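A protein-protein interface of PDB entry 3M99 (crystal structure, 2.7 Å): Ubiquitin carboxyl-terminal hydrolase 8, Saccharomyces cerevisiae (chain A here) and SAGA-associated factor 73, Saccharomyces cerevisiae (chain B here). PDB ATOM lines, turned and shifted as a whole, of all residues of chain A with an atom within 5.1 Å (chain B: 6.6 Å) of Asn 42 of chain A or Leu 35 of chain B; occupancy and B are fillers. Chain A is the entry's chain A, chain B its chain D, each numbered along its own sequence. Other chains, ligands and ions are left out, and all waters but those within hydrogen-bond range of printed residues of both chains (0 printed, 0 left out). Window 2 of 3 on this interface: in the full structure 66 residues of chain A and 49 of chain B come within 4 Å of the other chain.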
ATOM      1  N   ILE A  30     -31.558  24.922 -15.698  1.00  0.00           N
ATOM      2  CA  ILE A  30     -30.130  24.913 -15.998  1.00  0.00           C
ATOM      3  C   ILE A  30     -29.682  23.558 -16.527  1.00  0.00           C
ATOM      4  O   ILE A  30     -28.768  23.474 -17.350  1.00  0.00           O
ATOM      5  CB  ILE A  30     -29.271  25.287 -14.777  1.00  0.00           C
ATOM      6  CG1 ILE A  30     -29.264  26.798 -14.571  1.00  0.00           C
ATOM      7  CG2 ILE A  30     -27.848  24.790 -14.953  1.00  0.00           C
ATOM      8  CD1 ILE A  30     -28.793  27.192 -13.202  1.00  0.00           C
ATOM      9  N   SER A  34     -28.013  23.202 -20.603  1.00  0.00           N
ATOM     10  CA  SER A  34     -26.594  23.212 -20.374  1.00  0.00           C
ATOM     11  C   SER A  34     -25.924  22.362 -21.428  1.00  0.00           C
ATOM     12  O   SER A  34     -26.331  21.232 -21.680  1.00  0.00           O
ATOM     13  CB  SER A  34     -26.295  22.673 -18.978  1.00  0.00           C
ATOM     14  OG  SER A  34     -24.901  22.636 -18.738  1.00  0.00           O
ATOM     15  N   GLU A  38     -20.262  21.921 -20.293  1.00  0.00           N
ATOM     16  CA  GLU A  38     -20.473  22.732 -19.112  1.00  0.00           C
ATOM     17  C   GLU A  38     -21.409  22.042 -18.128  1.00  0.00           C
ATOM     18  O   GLU A  38     -21.511  22.430 -16.962  1.00  0.00           O
ATOM     19  CB  GLU A  38     -20.987  24.112 -19.512  1.00  0.00           C
ATOM     20  CG  GLU A  38     -19.845  25.068 -19.835  1.00  0.00           C
ATOM     21  CD  GLU A  38     -20.311  26.459 -20.204  1.00  0.00           C
ATOM     22  OE1 GLU A  38     -21.329  26.579 -20.923  1.00  0.00           O
ATOM     23  OE2 GLU A  38     -19.649  27.432 -19.782  1.00  0.00           O
ATOM     24  N   LYS A  39     -22.079  21.003 -18.610  1.00  0.00           N
ATOM     25  CA  LYS A  39     -22.981  20.224 -17.788  1.00  0.00           C
ATOM     26  C   LYS A  39     -22.208  19.156 -17.032  1.00  0.00           C
ATOM     27  O   LYS A  39     -22.703  18.592 -16.064  1.00  0.00           O
ATOM     28  CB  LYS A  39     -24.065  19.599 -18.662  1.00  0.00           C
ATOM     29  CG  LYS A  39     -25.026  18.676 -17.944  1.00  0.00           C
ATOM     30  CD  LYS A  39     -26.389  18.760 -18.589  1.00  0.00           C
ATOM     31  CE  LYS A  39     -27.241  17.574 -18.221  1.00  0.00           C
ATOM     32  NZ  LYS A  39     -27.400  17.487 -16.755  1.00  0.00           N
ATOM     33  N   PHE A  40     -20.985  18.877 -17.467  1.00  0.00           N
ATOM     34  CA  PHE A  40     -20.125  17.965 -16.719  1.00  0.00           C
ATOM     35  C   PHE A  40     -19.289  18.700 -15.660  1.00  0.00           C
ATOM     36  O   PHE A  40     -19.312  18.343 -14.485  1.00  0.00           O
ATOM     37  CB  PHE A  40     -19.224  17.160 -17.657  1.00  0.00           C
ATOM     38  CG  PHE A  40     -19.933  16.046 -18.365  1.00  0.00           C
ATOM     39  CD1 PHE A  40     -19.934  15.969 -19.749  1.00  0.00           C
ATOM     40  CD2 PHE A  40     -20.605  15.078 -17.643  1.00  0.00           C
ATOM     41  CE1 PHE A  40     -20.582  14.944 -20.395  1.00  0.00           C
ATOM     42  CE2 PHE A  40     -21.256  14.053 -18.276  1.00  0.00           C
ATOM     43  CZ  PHE A  40     -21.248  13.983 -19.655  1.00  0.00           C
ATOM     44  N   LEU A  41     -18.576  19.740 -16.085  1.00  0.00           N
ATOM     45  CA  LEU A  41     -17.630  20.449 -15.228  1.00  0.00           C
ATOM     46  C   LEU A  41     -18.281  21.449 -14.277  1.00  0.00           C
ATOM     47  O   LEU A  41     -17.583  22.168 -13.559  1.00  0.00           O
ATOM     48  CB  LEU A  41     -16.603  21.192 -16.089  1.00  0.00           C
ATOM     49  CG  LEU A  41     -15.652  20.365 -16.951  1.00  0.00           C
ATOM     50  CD1 LEU A  41     -14.843  21.266 -17.868  1.00  0.00           C
ATOM     51  CD2 LEU A  41     -14.742  19.539 -16.067  1.00  0.00           C
ATOM     52  N   ASN A  42     -19.607  21.516 -14.274  1.00  0.00           N
ATOM     53  CA  ASN A  42     -20.291  22.484 -13.424  1.00  0.00           C
ATOM     54  C   ASN A  42     -21.345  21.866 -12.514  1.00  0.00           C
ATOM     55  O   ASN A  42     -21.585  22.352 -11.403  1.00  0.00           O
ATOM     56  CB  ASN A  42     -20.898  23.608 -14.263  1.00  0.00           C
ATOM     57  CG  ASN A  42     -19.841  24.522 -14.867  1.00  0.00           C
ATOM     58  OD1 ASN A  42     -19.001  25.076 -14.154  1.00  0.00           O
ATOM     59  ND2 ASN A  42     -19.884  24.689 -16.184  1.00  0.00           N
ATOM     60  N   THR A  43     -21.962  20.784 -12.978  1.00  0.00           N
ATOM     61  CA  THR A  43     -23.044  20.163 -12.228  1.00  0.00           C
ATOM     62  C   THR A  43     -22.769  18.703 -11.894  1.00  0.00           C
ATOM     63  O   THR A  43     -23.566  18.059 -11.230  1.00  0.00           O
ATOM     64  CB  THR A  43     -24.366  20.252 -12.993  1.00  0.00           C
ATOM     65  OG1 THR A  43     -24.292  19.424 -14.156  1.00  0.00           O
ATOM     66  CG2 THR A  43     -24.653  21.695 -13.414  1.00  0.00           C
ATOM     67  N   MET A  44     -21.640  18.182 -12.352  1.00  0.00           N
ATOM     68  CA  MET A  44     -21.280  16.798 -12.073  1.00  0.00           C
ATOM     69  C   MET A  44     -19.818  16.711 -11.686  1.00  0.00           C
ATOM     70  O   MET A  44     -19.172  15.682 -11.876  1.00  0.00           O
ATOM     71  CB  MET A  44     -21.543  15.919 -13.291  1.00  0.00           C
ATOM     72  CG  MET A  44     -22.948  16.061 -13.852  1.00  0.00           C
ATOM     73  SD  MET A  44     -23.350  14.825 -15.087  1.00  0.00           S
ATOM     74  CE  MET A  44     -25.138  14.921 -15.060  1.00  0.00           C
ATOM     75  N   LYS A  45     -19.305  17.819 -11.167  1.00  0.00           N
ATOM     76  CA  LYS A  45     -17.983  17.875 -10.573  1.00  0.00           C
ATOM     77  C   LYS A  45     -18.155  18.097  -9.077  1.00  0.00           C
ATOM     78  O   LYS A  45     -18.707  19.116  -8.659  1.00  0.00           O
ATOM     79  CB  LYS A  45     -17.204  19.040 -11.173  1.00  0.00           C
ATOM     80  CG  LYS A  45     -15.791  19.214 -10.641  1.00  0.00           C
ATOM     81  CD  LYS A  45     -15.061  20.294 -11.439  1.00  0.00           C
ATOM     82  CE  LYS A  45     -13.555  20.266 -11.204  1.00  0.00           C
ATOM     83  NZ  LYS A  45     -12.826  21.177 -12.143  1.00  0.00           N
ATOM     84  N   CYS A  66     -21.806  21.432  -5.065  1.00  0.00           N
ATOM     85  CA  CYS A  66     -22.150  20.194  -5.756  1.00  0.00           C
ATOM     86  C   CYS A  66     -21.304  19.072  -5.190  1.00  0.00           C
ATOM     87  O   CYS A  66     -20.079  19.104  -5.312  1.00  0.00           O
ATOM     88  CB  CYS A  66     -21.837  20.306  -7.248  1.00  0.00           C
ATOM     89  SG  CYS A  66     -22.966  21.338  -8.193  1.00  0.00           S
ATOM     90  N   ASP B  30     -16.986  26.994  -8.731  1.00  0.00           N
ATOM     91  CA  ASP B  30     -17.422  26.899  -7.343  1.00  0.00           C
ATOM     92  C   ASP B  30     -18.956  26.860  -7.178  1.00  0.00           C
ATOM     93  O   ASP B  30     -19.470  26.038  -6.416  1.00  0.00           O
ATOM     94  CB  ASP B  30     -16.785  28.005  -6.474  1.00  0.00           C
ATOM     95  CG  ASP B  30     -15.593  27.500  -5.636  1.00  0.00           C
ATOM     96  OD1 ASP B  30     -15.658  26.362  -5.118  1.00  0.00           O
ATOM     97  OD2 ASP B  30     -14.595  28.244  -5.478  1.00  0.00           O
ATOM     98  N   SER B  31     -19.689  27.715  -7.893  1.00  0.00           N
ATOM     99  CA  SER B  31     -21.149  27.804  -7.702  1.00  0.00           C
ATOM    100  C   SER B  31     -22.001  27.375  -8.911  1.00  0.00           C
ATOM    101  O   SER B  31     -21.802  27.871 -10.016  1.00  0.00           O
ATOM    102  CB  SER B  31     -21.534  29.226  -7.288  1.00  0.00           C
ATOM    103  OG  SER B  31     -22.935  29.354  -7.131  1.00  0.00           O
ATOM    104  N   TRP B  32     -22.967  26.480  -8.710  1.00  0.00           N
ATOM    105  CA  TRP B  32     -23.822  26.071  -9.831  1.00  0.00           C
ATOM    106  C   TRP B  32     -24.856  27.130 -10.199  1.00  0.00           C
ATOM    107  O   TRP B  32     -25.323  27.164 -11.333  1.00  0.00           O
ATOM    108  CB  TRP B  32     -24.531  24.731  -9.583  1.00  0.00           C
ATOM    109  CG  TRP B  32     -25.627  24.811  -8.560  1.00  0.00           C
ATOM    110  CD1 TRP B  32     -25.539  24.466  -7.245  1.00  0.00           C
ATOM    111  CD2 TRP B  32     -26.972  25.281  -8.763  1.00  0.00           C
ATOM    112  NE1 TRP B  32     -26.741  24.686  -6.616  1.00  0.00           N
ATOM    113  CE2 TRP B  32     -27.633  25.186  -7.520  1.00  0.00           C
ATOM    114  CE3 TRP B  32     -27.674  25.770  -9.866  1.00  0.00           C
ATOM    115  CZ2 TRP B  32     -28.968  25.562  -7.358  1.00  0.00           C
ATOM    116  CZ3 TRP B  32     -28.999  26.145  -9.698  1.00  0.00           C
ATOM    117  CH2 TRP B  32     -29.630  26.038  -8.453  1.00  0.00           C
ATOM    118  N   LYS B  33     -25.230  27.986  -9.255  1.00  0.00           N
ATOM    119  CA  LYS B  33     -26.231  29.009  -9.554  1.00  0.00           C
ATOM    120  C   LYS B  33     -25.703  30.064 -10.532  1.00  0.00           C
ATOM    121  O   LYS B  33     -26.433  30.980 -10.927  1.00  0.00           O
ATOM    122  CB  LYS B  33     -26.735  29.680  -8.277  1.00  0.00           C
ATOM    123  CG  LYS B  33     -27.533  28.771  -7.343  1.00  0.00           C
ATOM    124  CD  LYS B  33     -27.872  29.494  -6.038  1.00  0.00           C
ATOM    125  CE  LYS B  33     -28.839  28.703  -5.176  1.00  0.00           C
ATOM    126  NZ  LYS B  33     -29.251  29.475  -3.968  1.00  0.00           N
ATOM    127  N   SER B  34     -24.438  29.933 -10.924  1.00  0.00           N
ATOM    128  CA  SER B  34     -23.827  30.896 -11.833  1.00  0.00           C
ATOM    129  C   SER B  34     -24.046  30.545 -13.311  1.00  0.00           C
ATOM    130  O   SER B  34     -23.811  31.375 -14.193  1.00  0.00           O
ATOM    131  CB  SER B  34     -22.334  31.069 -11.523  1.00  0.00           C
ATOM    132  OG  SER B  34     -21.575  29.961 -11.976  1.00  0.00           O
ATOM    133  N   LEU B  35     -24.508  29.324 -13.577  1.00  0.00           N
ATOM    134  CA  LEU B  35     -24.773  28.887 -14.951  1.00  0.00           C
ATOM    135  C   LEU B  35     -26.027  29.522 -15.544  1.00  0.00           C
ATOM    136  O   LEU B  35     -26.205  29.524 -16.759  1.00  0.00           O
ATOM    137  CB  LEU B  35     -24.890  27.366 -15.037  1.00  0.00           C
ATOM    138  CG  LEU B  35     -23.655  26.546 -14.673  1.00  0.00           C
ATOM    139  CD1 LEU B  35     -23.928  25.078 -14.902  1.00  0.00           C
ATOM    140  CD2 LEU B  35     -22.477  26.995 -15.498  1.00  0.00           C
ATOM    141  N   MET B  36     -26.885  30.069 -14.690  1.00  0.00           N
ATOM    142  CA  MET B  36     -28.146  30.638 -15.142  1.00  0.00           C
ATOM    143  C   MET B  36     -27.980  31.701 -16.227  1.00  0.00           C
ATOM    144  O   MET B  36     -28.886  31.912 -17.030  1.00  0.00           O
ATOM    145  CB  MET B  36     -28.938  31.201 -13.967  1.00  0.00           C
ATOM    146  CG  MET B  36     -30.332  31.701 -14.320  1.00  0.00           C
ATOM    147  SD  MET B  36     -31.437  30.475 -15.076  1.00  0.00           S
ATOM    148  CE  MET B  36     -31.533  29.206 -13.814  1.00  0.00           C
ATOM    149  N   SER B  37     -26.832  32.367 -16.270  1.00  0.00           N
ATOM    150  CA  SER B  37     -26.631  33.432 -17.252  1.00  0.00           C
ATOM    151  C   SER B  37     -26.565  32.909 -18.696  1.00  0.00           C
ATOM    152  O   SER B  37     -27.208  33.451 -19.599  1.00  0.00           O
ATOM    153  CB  SER B  37     -25.345  34.205 -16.949  1.00  0.00           C
ATOM    154  OG  SER B  37     -25.139  35.240 -17.893  1.00  0.00           O
ATOM    155  N   SER B  38     -25.792  31.849 -18.905  1.00  0.00           N
ATOM    156  CA  SER B  38     -25.643  31.275 -20.230  1.00  0.00           C
ATOM    157  C   SER B  38     -26.675  30.185 -20.501  1.00  0.00           C
ATOM    158  O   SER B  38     -27.038  29.940 -21.648  1.00  0.00           O
ATOM    159  CB  SER B  38     -24.228  30.732 -20.425  1.00  0.00           C
ATOM    160  OG  SER B  38     -23.986  29.634 -19.572  1.00  0.00           O
ATOM    161  N   ALA B  39     -27.152  29.528 -19.451  1.00  0.00           N
ATOM    162  CA  ALA B  39     -28.220  28.551 -19.619  1.00  0.00           C
ATOM    163  C   ALA B  39     -29.465  29.224 -20.190  1.00  0.00           C
ATOM    164  O   ALA B  39     -30.355  28.557 -20.695  1.00  0.00           O
ATOM    165  CB  ALA B  39     -28.539  27.882 -18.310  1.00  0.00           C
ATOM    166  N   LYS B  40     -29.527  30.547 -20.109  1.00  0.00           N
ATOM    167  CA  LYS B  40     -30.655  31.287 -20.662  1.00  0.00           C
ATOM    168  C   LYS B  40     -30.328  31.720 -22.079  1.00  0.00           C
ATOM    169  O   LYS B  40     -31.219  31.985 -22.882  1.00  0.00           O
ATOM    170  CB  LYS B  40     -30.985  32.509 -19.798  1.00  0.00           C
ATOM    171  CG  LYS B  40     -31.772  32.187 -18.520  1.00  0.00           C
ATOM    172  CD  LYS B  40     -32.199  33.439 -17.748  1.00  0.00           C
ATOM    173  CE  LYS B  40     -31.034  34.046 -16.979  1.00  0.00           C
ATOM    174  NZ  LYS B  40     -31.373  35.316 -16.262  1.00  0.00           N
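The backbone carbonyl oxygen of Asn 42 of chain A lies within hydrogen-bond range of the side-chain sulfur of Cys 66 of chain A, 3.6 Å away. The side-chain amide nitrogen (ND2) of Asn 42 of chain A sits at hydrogen-bond distance from the backbone carbonyl oxygen (O) of Glu 38 of chain A, 2.9 Å away. The backbone carbonyl oxygen of Lys 39 of chain A sits at hydrogen-bond distance from the side-chain hydroxyl of Thr 43 of chain A, at 2.6 Å.
Among the printed residues, merely in contact across the chains: Ile 30 of chain A with Met 36 of chain B, Asn 42 of chain A with Leu 35 of chain B, Ile 30 of chain A with Trp 32 of chain B, Thr 43 of chain A with Leu 35 of chain B, Ile 30 of chain A with Leu 35 of chain B, Ile 30 of chain A with Ala 39 of chain B and Cys 66 of chain A with Trp 32 of chain B.
Of the printed residues of chain B, Ile 30 of chain A touches Trp 32 (3.7 Å), Leu 35 (3.9 Å), Met 36 (3.4 Å) and Ala 39 (3.96 Å). Printed residues of chain B within 4 Å of Cys 66 of chain A: Trp 32 (3.99 Å). Ser 34 of chain B touches none of the printed residues of chain A. Of chain A, only Ile 30 (3.9 Å), Asn 42 (3.4 Å) and Thr 43 (3.8 Å) come within 4 Å of Leu 35 of chain B. Ser 37 of chain B touches none of the printed residues of chain A. The nearest residue of chain B that does not touch Asn 42 of chain A is Trp 32 of chain B (4.2 Å). The nearest residue of chain A that does not touch Leu 35 of chain B is Glu 38 of chain A (4.1 Å).
Of the 11 printed residues of chain A, 4 touch a printed residue of chain B. Hydrophobic or aromatic side chains of chain A that line the printed part of chain B: Ile 30. Hydrophobic or aromatic side chains of chain B within 4 Å of the printed part of chain A: Trp 32, Leu 35, Met 36 and Ala 39. Among the printed residues, 7 pairs touch across the chains. Among the printed residues, no Asp or Glu carboxylate lies within 4 Å of a Lys or Arg side-chain nitrogen of the other chain.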
